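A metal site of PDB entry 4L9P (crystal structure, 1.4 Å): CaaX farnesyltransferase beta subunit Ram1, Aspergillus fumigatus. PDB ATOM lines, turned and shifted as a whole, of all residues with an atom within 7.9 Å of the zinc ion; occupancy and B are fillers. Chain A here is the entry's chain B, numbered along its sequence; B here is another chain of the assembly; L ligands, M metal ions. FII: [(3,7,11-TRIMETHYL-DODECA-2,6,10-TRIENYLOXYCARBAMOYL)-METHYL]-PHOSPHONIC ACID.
OD1 of Asp 430 is in hydrogen-bond range of N of His 433 (2.7 Å).
The side-chain hydroxyl (OH) of Tyr 432 lies close to the side-chain sulfur (SG) of Cys 367.
The indole nitrogen (NE1) of Trp 371 is in hydrogen-bond range of the side-chain hydroxyl (OH) of Tyr 432.
The side-chain carboxylate (OD1) of Asp 430 is in hydrogen-bond range of the backbone NH (N) of Tyr 432 (3.1 Å).
The zinc ion is bound by OD2 of Asp 365 (2.0 Å), NE2 of His 433 (2.0 Å), SG of Cys 2 of chain B (2.3 Å), SG of Cys 367 (2.4 Å) and OD1 of Asp 365 (2.6 Å).
Merely in contact with the zinc ion: Tyr 432.
Of the 18 residues printed, 5 come within 4 Å of the zinc ion.
The nearest printed residue that does not touch the zinc ion is Asp 423 (4.3 Å).
OH of Tyr 368 lies within hydrogen-bond range of O51 of the ligand.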
ATOM      1  N   VAL A 364     -35.704 -16.627  -8.340  1.00  0.00           N
ATOM      2  CA  VAL A 364     -34.628 -15.730  -8.796  1.00  0.00           C
ATOM      3  C   VAL A 364     -34.441 -14.517  -7.886  1.00  0.00           C
ATOM      4  O   VAL A 364     -35.366 -14.077  -7.197  1.00  0.00           O
ATOM      5  CB  VAL A 364     -34.855 -15.269 -10.251  1.00  0.00           C
ATOM      6  CG1 VAL A 364     -34.825 -16.488 -11.199  1.00  0.00           C
ATOM      7  CG2 VAL A 364     -36.123 -14.420 -10.384  1.00  0.00           C
ATOM      8  N   ASP A 365     -33.232 -13.949  -7.904  1.00  0.00           N
ATOM      9  CA  ASP A 365     -32.940 -12.747  -7.127  1.00  0.00           C
ATOM     10  C   ASP A 365     -31.696 -12.104  -7.735  1.00  0.00           C
ATOM     11  O   ASP A 365     -30.696 -12.784  -8.030  1.00  0.00           O
ATOM     12  CB  ASP A 365     -32.682 -13.204  -5.641  1.00  0.00           C
ATOM     13  CG  ASP A 365     -32.199 -12.147  -4.741  1.00  0.00           C
ATOM     14  OD1 ASP A 365     -31.767 -11.039  -5.149  1.00  0.00           O
ATOM     15  OD2 ASP A 365     -32.251 -12.357  -3.521  1.00  0.00           O
ATOM     16  N   GLY A 366     -31.823 -10.815  -7.984  1.00  0.00           N
ATOM     17  CA  GLY A 366     -30.722 -10.074  -8.623  1.00  0.00           C
ATOM     18  C   GLY A 366     -29.398 -10.171  -7.875  1.00  0.00           C
ATOM     19  O   GLY A 366     -28.344  -9.994  -8.526  1.00  0.00           O
ATOM     20  N   CYS A 367     -29.361 -10.428  -6.545  1.00  0.00           N
ATOM     21  CA  CYS A 367     -28.005 -10.479  -5.952  1.00  0.00           C
ATOM     22  C   CYS A 367     -27.216 -11.732  -6.380  1.00  0.00           C
ATOM     23  O   CYS A 367     -25.971 -11.720  -6.354  1.00  0.00           O
ATOM     24  CB  CYS A 367     -28.038 -10.343  -4.392  1.00  0.00           C
ATOM     25  SG  CYS A 367     -28.880 -11.797  -3.541  1.00  0.00           S
ATOM     26  N   TYR A 368     -27.948 -12.756  -6.826  1.00  0.00           N
ATOM     27  CA  TYR A 368     -27.248 -13.954  -7.328  1.00  0.00           C
ATOM     28  C   TYR A 368     -26.580 -13.652  -8.679  1.00  0.00           C
ATOM     29  O   TYR A 368     -25.832 -14.482  -9.159  1.00  0.00           O
ATOM     30  CB  TYR A 368     -28.183 -15.192  -7.405  1.00  0.00           C
ATOM     31  CG  TYR A 368     -28.725 -15.548  -6.006  1.00  0.00           C
ATOM     32  CD1 TYR A 368     -27.839 -15.604  -4.920  1.00  0.00           C
ATOM     33  CD2 TYR A 368     -30.070 -15.707  -5.799  1.00  0.00           C
ATOM     34  CE1 TYR A 368     -28.318 -15.864  -3.591  1.00  0.00           C
ATOM     35  CE2 TYR A 368     -30.580 -15.979  -4.522  1.00  0.00           C
ATOM     36  CZ  TYR A 368     -29.683 -16.009  -3.450  1.00  0.00           C
ATOM     37  OH  TYR A 368     -30.152 -16.289  -2.176  1.00  0.00           O
ATOM     38  N   SER A 369     -26.904 -12.499  -9.287  1.00  0.00           N
ATOM     39  CA  SER A 369     -26.145 -12.137 -10.476  1.00  0.00           C
ATOM     40  C   SER A 369     -24.657 -12.114 -10.167  1.00  0.00           C
ATOM     41  O   SER A 369     -23.829 -12.490 -11.039  1.00  0.00           O
ATOM     42  CB  SER A 369     -26.573 -10.732 -10.935  1.00  0.00           C
ATOM     43  OG  SER A 369     -27.970 -10.696 -11.083  1.00  0.00           O
ATOM     44  N   TRP A 371     -23.460 -13.799  -6.924  1.00  0.00           N
ATOM     45  CA  TRP A 371     -23.005 -15.037  -6.223  1.00  0.00           C
ATOM     46  C   TRP A 371     -22.983 -16.223  -7.188  1.00  0.00           C
ATOM     47  O   TRP A 371     -22.047 -17.032  -7.120  1.00  0.00           O
ATOM     48  CB  TRP A 371     -23.934 -15.365  -5.035  1.00  0.00           C
ATOM     49  CG  TRP A 371     -23.985 -14.242  -4.013  1.00  0.00           C
ATOM     50  CD1 TRP A 371     -25.074 -13.453  -3.702  1.00  0.00           C
ATOM     51  CD2 TRP A 371     -22.907 -13.749  -3.229  1.00  0.00           C
ATOM     52  NE1 TRP A 371     -24.739 -12.499  -2.775  1.00  0.00           N
ATOM     53  CE2 TRP A 371     -23.401 -12.646  -2.456  1.00  0.00           C
ATOM     54  CE3 TRP A 371     -21.584 -14.127  -3.078  1.00  0.00           C
ATOM     55  CZ2 TRP A 371     -22.591 -11.901  -1.592  1.00  0.00           C
ATOM     56  CZ3 TRP A 371     -20.765 -13.393  -2.234  1.00  0.00           C
ATOM     57  CH2 TRP A 371     -21.294 -12.300  -1.471  1.00  0.00           C
ATOM     58  N   ARG A 422     -32.800  -4.000  -7.205  1.00  0.00           N
ATOM     59  CA  ARG A 422     -33.563  -4.809  -6.244  1.00  0.00           C
ATOM     60  C   ARG A 422     -33.400  -6.293  -6.528  1.00  0.00           C
ATOM     61  O   ARG A 422     -32.953  -6.742  -7.599  1.00  0.00           O
ATOM     62  CB  ARG A 422     -35.058  -4.388  -6.333  1.00  0.00           C
ATOM     63  CG  ARG A 422     -35.651  -4.665  -7.727  1.00  0.00           C
ATOM     64  CD  ARG A 422     -37.048  -4.025  -7.889  1.00  0.00           C
ATOM     65  NE  ARG A 422     -37.500  -4.151  -9.271  1.00  0.00           N
ATOM     66  CZ  ARG A 422     -38.187  -3.203  -9.907  1.00  0.00           C
ATOM     67  NH1 ARG A 422     -38.613  -2.119  -9.234  1.00  0.00           N
ATOM     68  NH2 ARG A 422     -38.504  -3.369 -11.183  1.00  0.00           N
ATOM     69  N   ASP A 423     -33.848  -7.053  -5.528  1.00  0.00           N
ATOM     70  CA  ASP A 423     -33.924  -8.499  -5.643  1.00  0.00           C
ATOM     71  C   ASP A 423     -34.784  -8.944  -6.810  1.00  0.00           C
ATOM     72  O   ASP A 423     -34.358  -9.661  -7.720  1.00  0.00           O
ATOM     73  CB  ASP A 423     -34.422  -8.992  -4.234  1.00  0.00           C
ATOM     74  CG  ASP A 423     -35.100 -10.346  -4.205  1.00  0.00           C
ATOM     75  OD1 ASP A 423     -35.158 -11.065  -5.199  1.00  0.00           O
ATOM     76  OD2 ASP A 423     -35.586 -10.713  -3.085  1.00  0.00           O
ATOM     77  N   LYS A 424     -36.006  -8.428  -6.824  1.00  0.00           N
ATOM     78  CA  LYS A 424     -36.965  -8.811  -7.853  1.00  0.00           C
ATOM     79  C   LYS A 424     -38.076  -7.763  -7.854  1.00  0.00           C
ATOM     80  O   LYS A 424     -38.187  -6.996  -6.905  1.00  0.00           O
ATOM     81  CB  LYS A 424     -37.523 -10.244  -7.604  1.00  0.00           C
ATOM     82  CG  LYS A 424     -38.339 -10.379  -6.295  1.00  0.00           C
ATOM     83  CD  LYS A 424     -39.029 -11.789  -6.236  1.00  0.00           C
ATOM     84  CE  LYS A 424     -38.078 -12.968  -6.306  1.00  0.00           C
ATOM     85  NZ  LYS A 424     -37.095 -12.998  -5.128  1.00  0.00           N
ATOM     86  N   ASP A 430     -32.057  -1.864  -2.293  1.00  0.00           N
ATOM     87  CA  ASP A 430     -31.139  -1.570  -1.192  1.00  0.00           C
ATOM     88  C   ASP A 430     -29.730  -1.577  -1.784  1.00  0.00           C
ATOM     89  O   ASP A 430     -29.523  -1.998  -2.933  1.00  0.00           O
ATOM     90  CB  ASP A 430     -31.328  -2.568  -0.024  1.00  0.00           C
ATOM     91  CG  ASP A 430     -31.113  -4.014  -0.463  1.00  0.00           C
ATOM     92  OD1 ASP A 430     -30.071  -4.342  -0.949  1.00  0.00           O
ATOM     93  OD2 ASP A 430     -31.985  -4.832  -0.256  1.00  0.00           O
ATOM     94  N   TYR A 432     -27.105  -3.337  -1.045  1.00  0.00           N
ATOM     95  CA  TYR A 432     -26.593  -4.725  -1.249  1.00  0.00           C
ATOM     96  C   TYR A 432     -27.049  -5.233  -2.620  1.00  0.00           C
ATOM     97  O   TYR A 432     -26.205  -5.720  -3.428  1.00  0.00           O
ATOM     98  CB  TYR A 432     -27.091  -5.638  -0.110  1.00  0.00           C
ATOM     99  CG  TYR A 432     -27.020  -7.102  -0.361  1.00  0.00           C
ATOM    100  CD1 TYR A 432     -25.849  -7.844  -0.050  1.00  0.00           C
ATOM    101  CD2 TYR A 432     -28.103  -7.779  -0.932  1.00  0.00           C
ATOM    102  CE1 TYR A 432     -25.792  -9.205  -0.314  1.00  0.00           C
ATOM    103  CE2 TYR A 432     -28.050  -9.146  -1.175  1.00  0.00           C
ATOM    104  CZ  TYR A 432     -26.899  -9.858  -0.873  1.00  0.00           C
ATOM    105  OH  TYR A 432     -26.875 -11.208  -1.198  1.00  0.00           O
ATOM    106  N   HIS A 433     -28.358  -5.142  -2.905  1.00  0.00           N
ATOM    107  CA  HIS A 433     -28.869  -5.576  -4.206  1.00  0.00           C
ATOM    108  C   HIS A 433     -28.329  -4.694  -5.339  1.00  0.00           C
ATOM    109  O   HIS A 433     -28.132  -5.194  -6.464  1.00  0.00           O
ATOM    110  CB  HIS A 433     -30.395  -5.671  -4.188  1.00  0.00           C
ATOM    111  CG  HIS A 433     -30.829  -6.932  -3.482  1.00  0.00           C
ATOM    112  ND1 HIS A 433     -31.248  -6.950  -2.167  1.00  0.00           N
ATOM    113  CD2 HIS A 433     -30.813  -8.221  -3.924  1.00  0.00           C
ATOM    114  CE1 HIS A 433     -31.469  -8.228  -1.819  1.00  0.00           C
ATOM    115  NE2 HIS A 433     -31.191  -9.005  -2.860  1.00  0.00           N
ATOM    116  N   TYR A 436     -24.626  -5.921  -5.978  1.00  0.00           N
ATOM    117  CA  TYR A 436     -24.440  -7.231  -6.588  1.00  0.00           C
ATOM    118  C   TYR A 436     -25.145  -7.397  -7.947  1.00  0.00           C
ATOM    119  O   TYR A 436     -24.623  -8.126  -8.785  1.00  0.00           O
ATOM    120  CB  TYR A 436     -24.791  -8.366  -5.598  1.00  0.00           C
ATOM    121  CG  TYR A 436     -23.738  -8.402  -4.491  1.00  0.00           C
ATOM    122  CD1 TYR A 436     -22.354  -8.561  -4.779  1.00  0.00           C
ATOM    123  CD2 TYR A 436     -24.098  -8.253  -3.158  1.00  0.00           C
ATOM    124  CE1 TYR A 436     -21.391  -8.640  -3.792  1.00  0.00           C
ATOM    125  CE2 TYR A 436     -23.147  -8.305  -2.166  1.00  0.00           C
ATOM    126  CZ  TYR A 436     -21.808  -8.500  -2.449  1.00  0.00           C
ATOM    127  OH  TYR A 436     -20.844  -8.542  -1.442  1.00  0.00           O
ATOM    128  N   LYS B   1     -35.931 -10.480   1.464  1.00  0.00           N
ATOM    129  CA  LYS B   1     -34.905  -9.950   2.371  1.00  0.00           C
ATOM    130  C   LYS B   1     -33.699 -10.867   2.445  1.00  0.00           C
ATOM    131  O   LYS B   1     -33.840 -12.062   2.732  1.00  0.00           O
ATOM    132  CB  LYS B   1     -35.441  -9.825   3.776  1.00  0.00           C
ATOM    133  CG  LYS B   1     -34.591  -8.868   4.605  1.00  0.00           C
ATOM    134  CD  LYS B   1     -34.217  -9.492   5.909  1.00  0.00           C
ATOM    135  CE  LYS B   1     -34.000  -8.417   6.963  1.00  0.00           C
ATOM    136  NZ  LYS B   1     -33.112  -7.330   6.425  1.00  0.00           N
ATOM    137  N   CYS B   2     -32.519 -10.300   2.191  1.00  0.00           N
ATOM    138  CA  CYS B   2     -31.308 -11.092   2.139  1.00  0.00           C
ATOM    139  C   CYS B   2     -30.471 -10.728   3.350  1.00  0.00           C
ATOM    140  O   CYS B   2     -30.461  -9.570   3.786  1.00  0.00           O
ATOM    141  CB  CYS B   2     -30.570 -10.853   0.818  1.00  0.00           C
ATOM    142  SG  CYS B   2     -31.489 -11.536  -0.541  1.00  0.00           S
ATOM    143  N   VAL B   3     -29.797 -11.703   3.901  1.00  0.00           N
ATOM    144  CA  VAL B   3     -29.005 -11.466   5.093  1.00  0.00           C
ATOM    145  C   VAL B   3     -27.732 -12.195   4.773  1.00  0.00           C
ATOM    146  O   VAL B   3     -27.814 -13.239   4.184  1.00  0.00           O
ATOM    147  CB  VAL B   3     -29.704 -12.092   6.300  1.00  0.00           C
ATOM    148  CG1 VAL B   3     -28.801 -12.204   7.553  1.00  0.00           C
ATOM    149  CG2 VAL B   3     -30.980 -11.277   6.651  1.00  0.00           C
ATOM    150  N   VAL B   4     -26.582 -11.600   5.119  1.00  0.00           N
ATOM    151  CA  VAL B   4     -25.261 -12.172   4.902  1.00  0.00           C
ATOM    152  C   VAL B   4     -24.446 -12.365   6.188  1.00  0.00           C
ATOM    153  O   VAL B   4     -23.400 -12.997   6.135  1.00  0.00           O
ATOM    154  CB  VAL B   4     -24.410 -11.366   3.905  1.00  0.00           C
ATOM    155  CG1 VAL B   4     -25.200 -11.122   2.662  1.00  0.00           C
ATOM    156  CG2 VAL B   4     -24.063 -10.022   4.453  1.00  0.00           C
HETATM  157  C1  FII L   1     -19.056 -13.140   1.478  1.00  0.00           C
HETATM  158  C2  FII L   1     -20.419 -13.422   2.045  1.00  0.00           C
HETATM  159  C6  FII L   1     -20.660 -12.917   3.407  1.00  0.00           C
HETATM  160  C10 FII L   1     -21.228 -14.474   1.416  1.00  0.00           C
HETATM  161  C11 FII L   1     -22.596 -14.929   1.926  1.00  0.00           C
HETATM  162  C12 FII L   1     -23.679 -14.214   1.069  1.00  0.00           C
HETATM  163  C15 FII L   1     -25.081 -14.815   1.072  1.00  0.00           C
HETATM  164  C18 FII L   1     -26.177 -14.155   0.245  1.00  0.00           C
HETATM  165  C22 FII L   1     -25.387 -15.732   2.205  1.00  0.00           C
HETATM  166  C23 FII L   1     -26.613 -16.606   2.002  1.00  0.00           C
HETATM  167  C24 FII L   1     -27.018 -17.295   3.251  1.00  0.00           C
HETATM  168  C27 FII L   1     -28.427 -17.767   3.155  1.00  0.00           C
HETATM  169  C30 FII L   1     -28.610 -19.165   2.588  1.00  0.00           C
HETATM  170  C34 FII L   1     -29.347 -17.196   4.172  1.00  0.00           C
HETATM  171  C35 FII L   1     -30.734 -17.746   4.423  1.00  0.00           C
HETATM  172  O36 FII L   1     -31.729 -16.807   4.038  1.00  0.00           O
HETATM  173  N42 FII L   1     -31.667 -16.361   2.750  1.00  0.00           N
HETATM  174  C43 FII L   1     -32.605 -17.005   1.921  1.00  0.00           C
HETATM  175  O44 FII L   1     -33.374 -17.913   2.276  1.00  0.00           O
HETATM  176  C45 FII L   1     -32.599 -16.457   0.503  1.00  0.00           C
HETATM  177  P46 FII L   1     -33.003 -17.731  -0.806  1.00  0.00           P
HETATM  178  O49 FII L   1     -32.170 -18.920  -0.487  1.00  0.00           O
HETATM  179  O50 FII L   1     -34.479 -17.950  -0.792  1.00  0.00           O
HETATM  180  O51 FII L   1     -32.543 -17.018  -2.094  1.00  0.00           O
HETATM  181 ZN    ZN M   1     -30.949 -11.026  -2.715  1.00  0.00          ZN
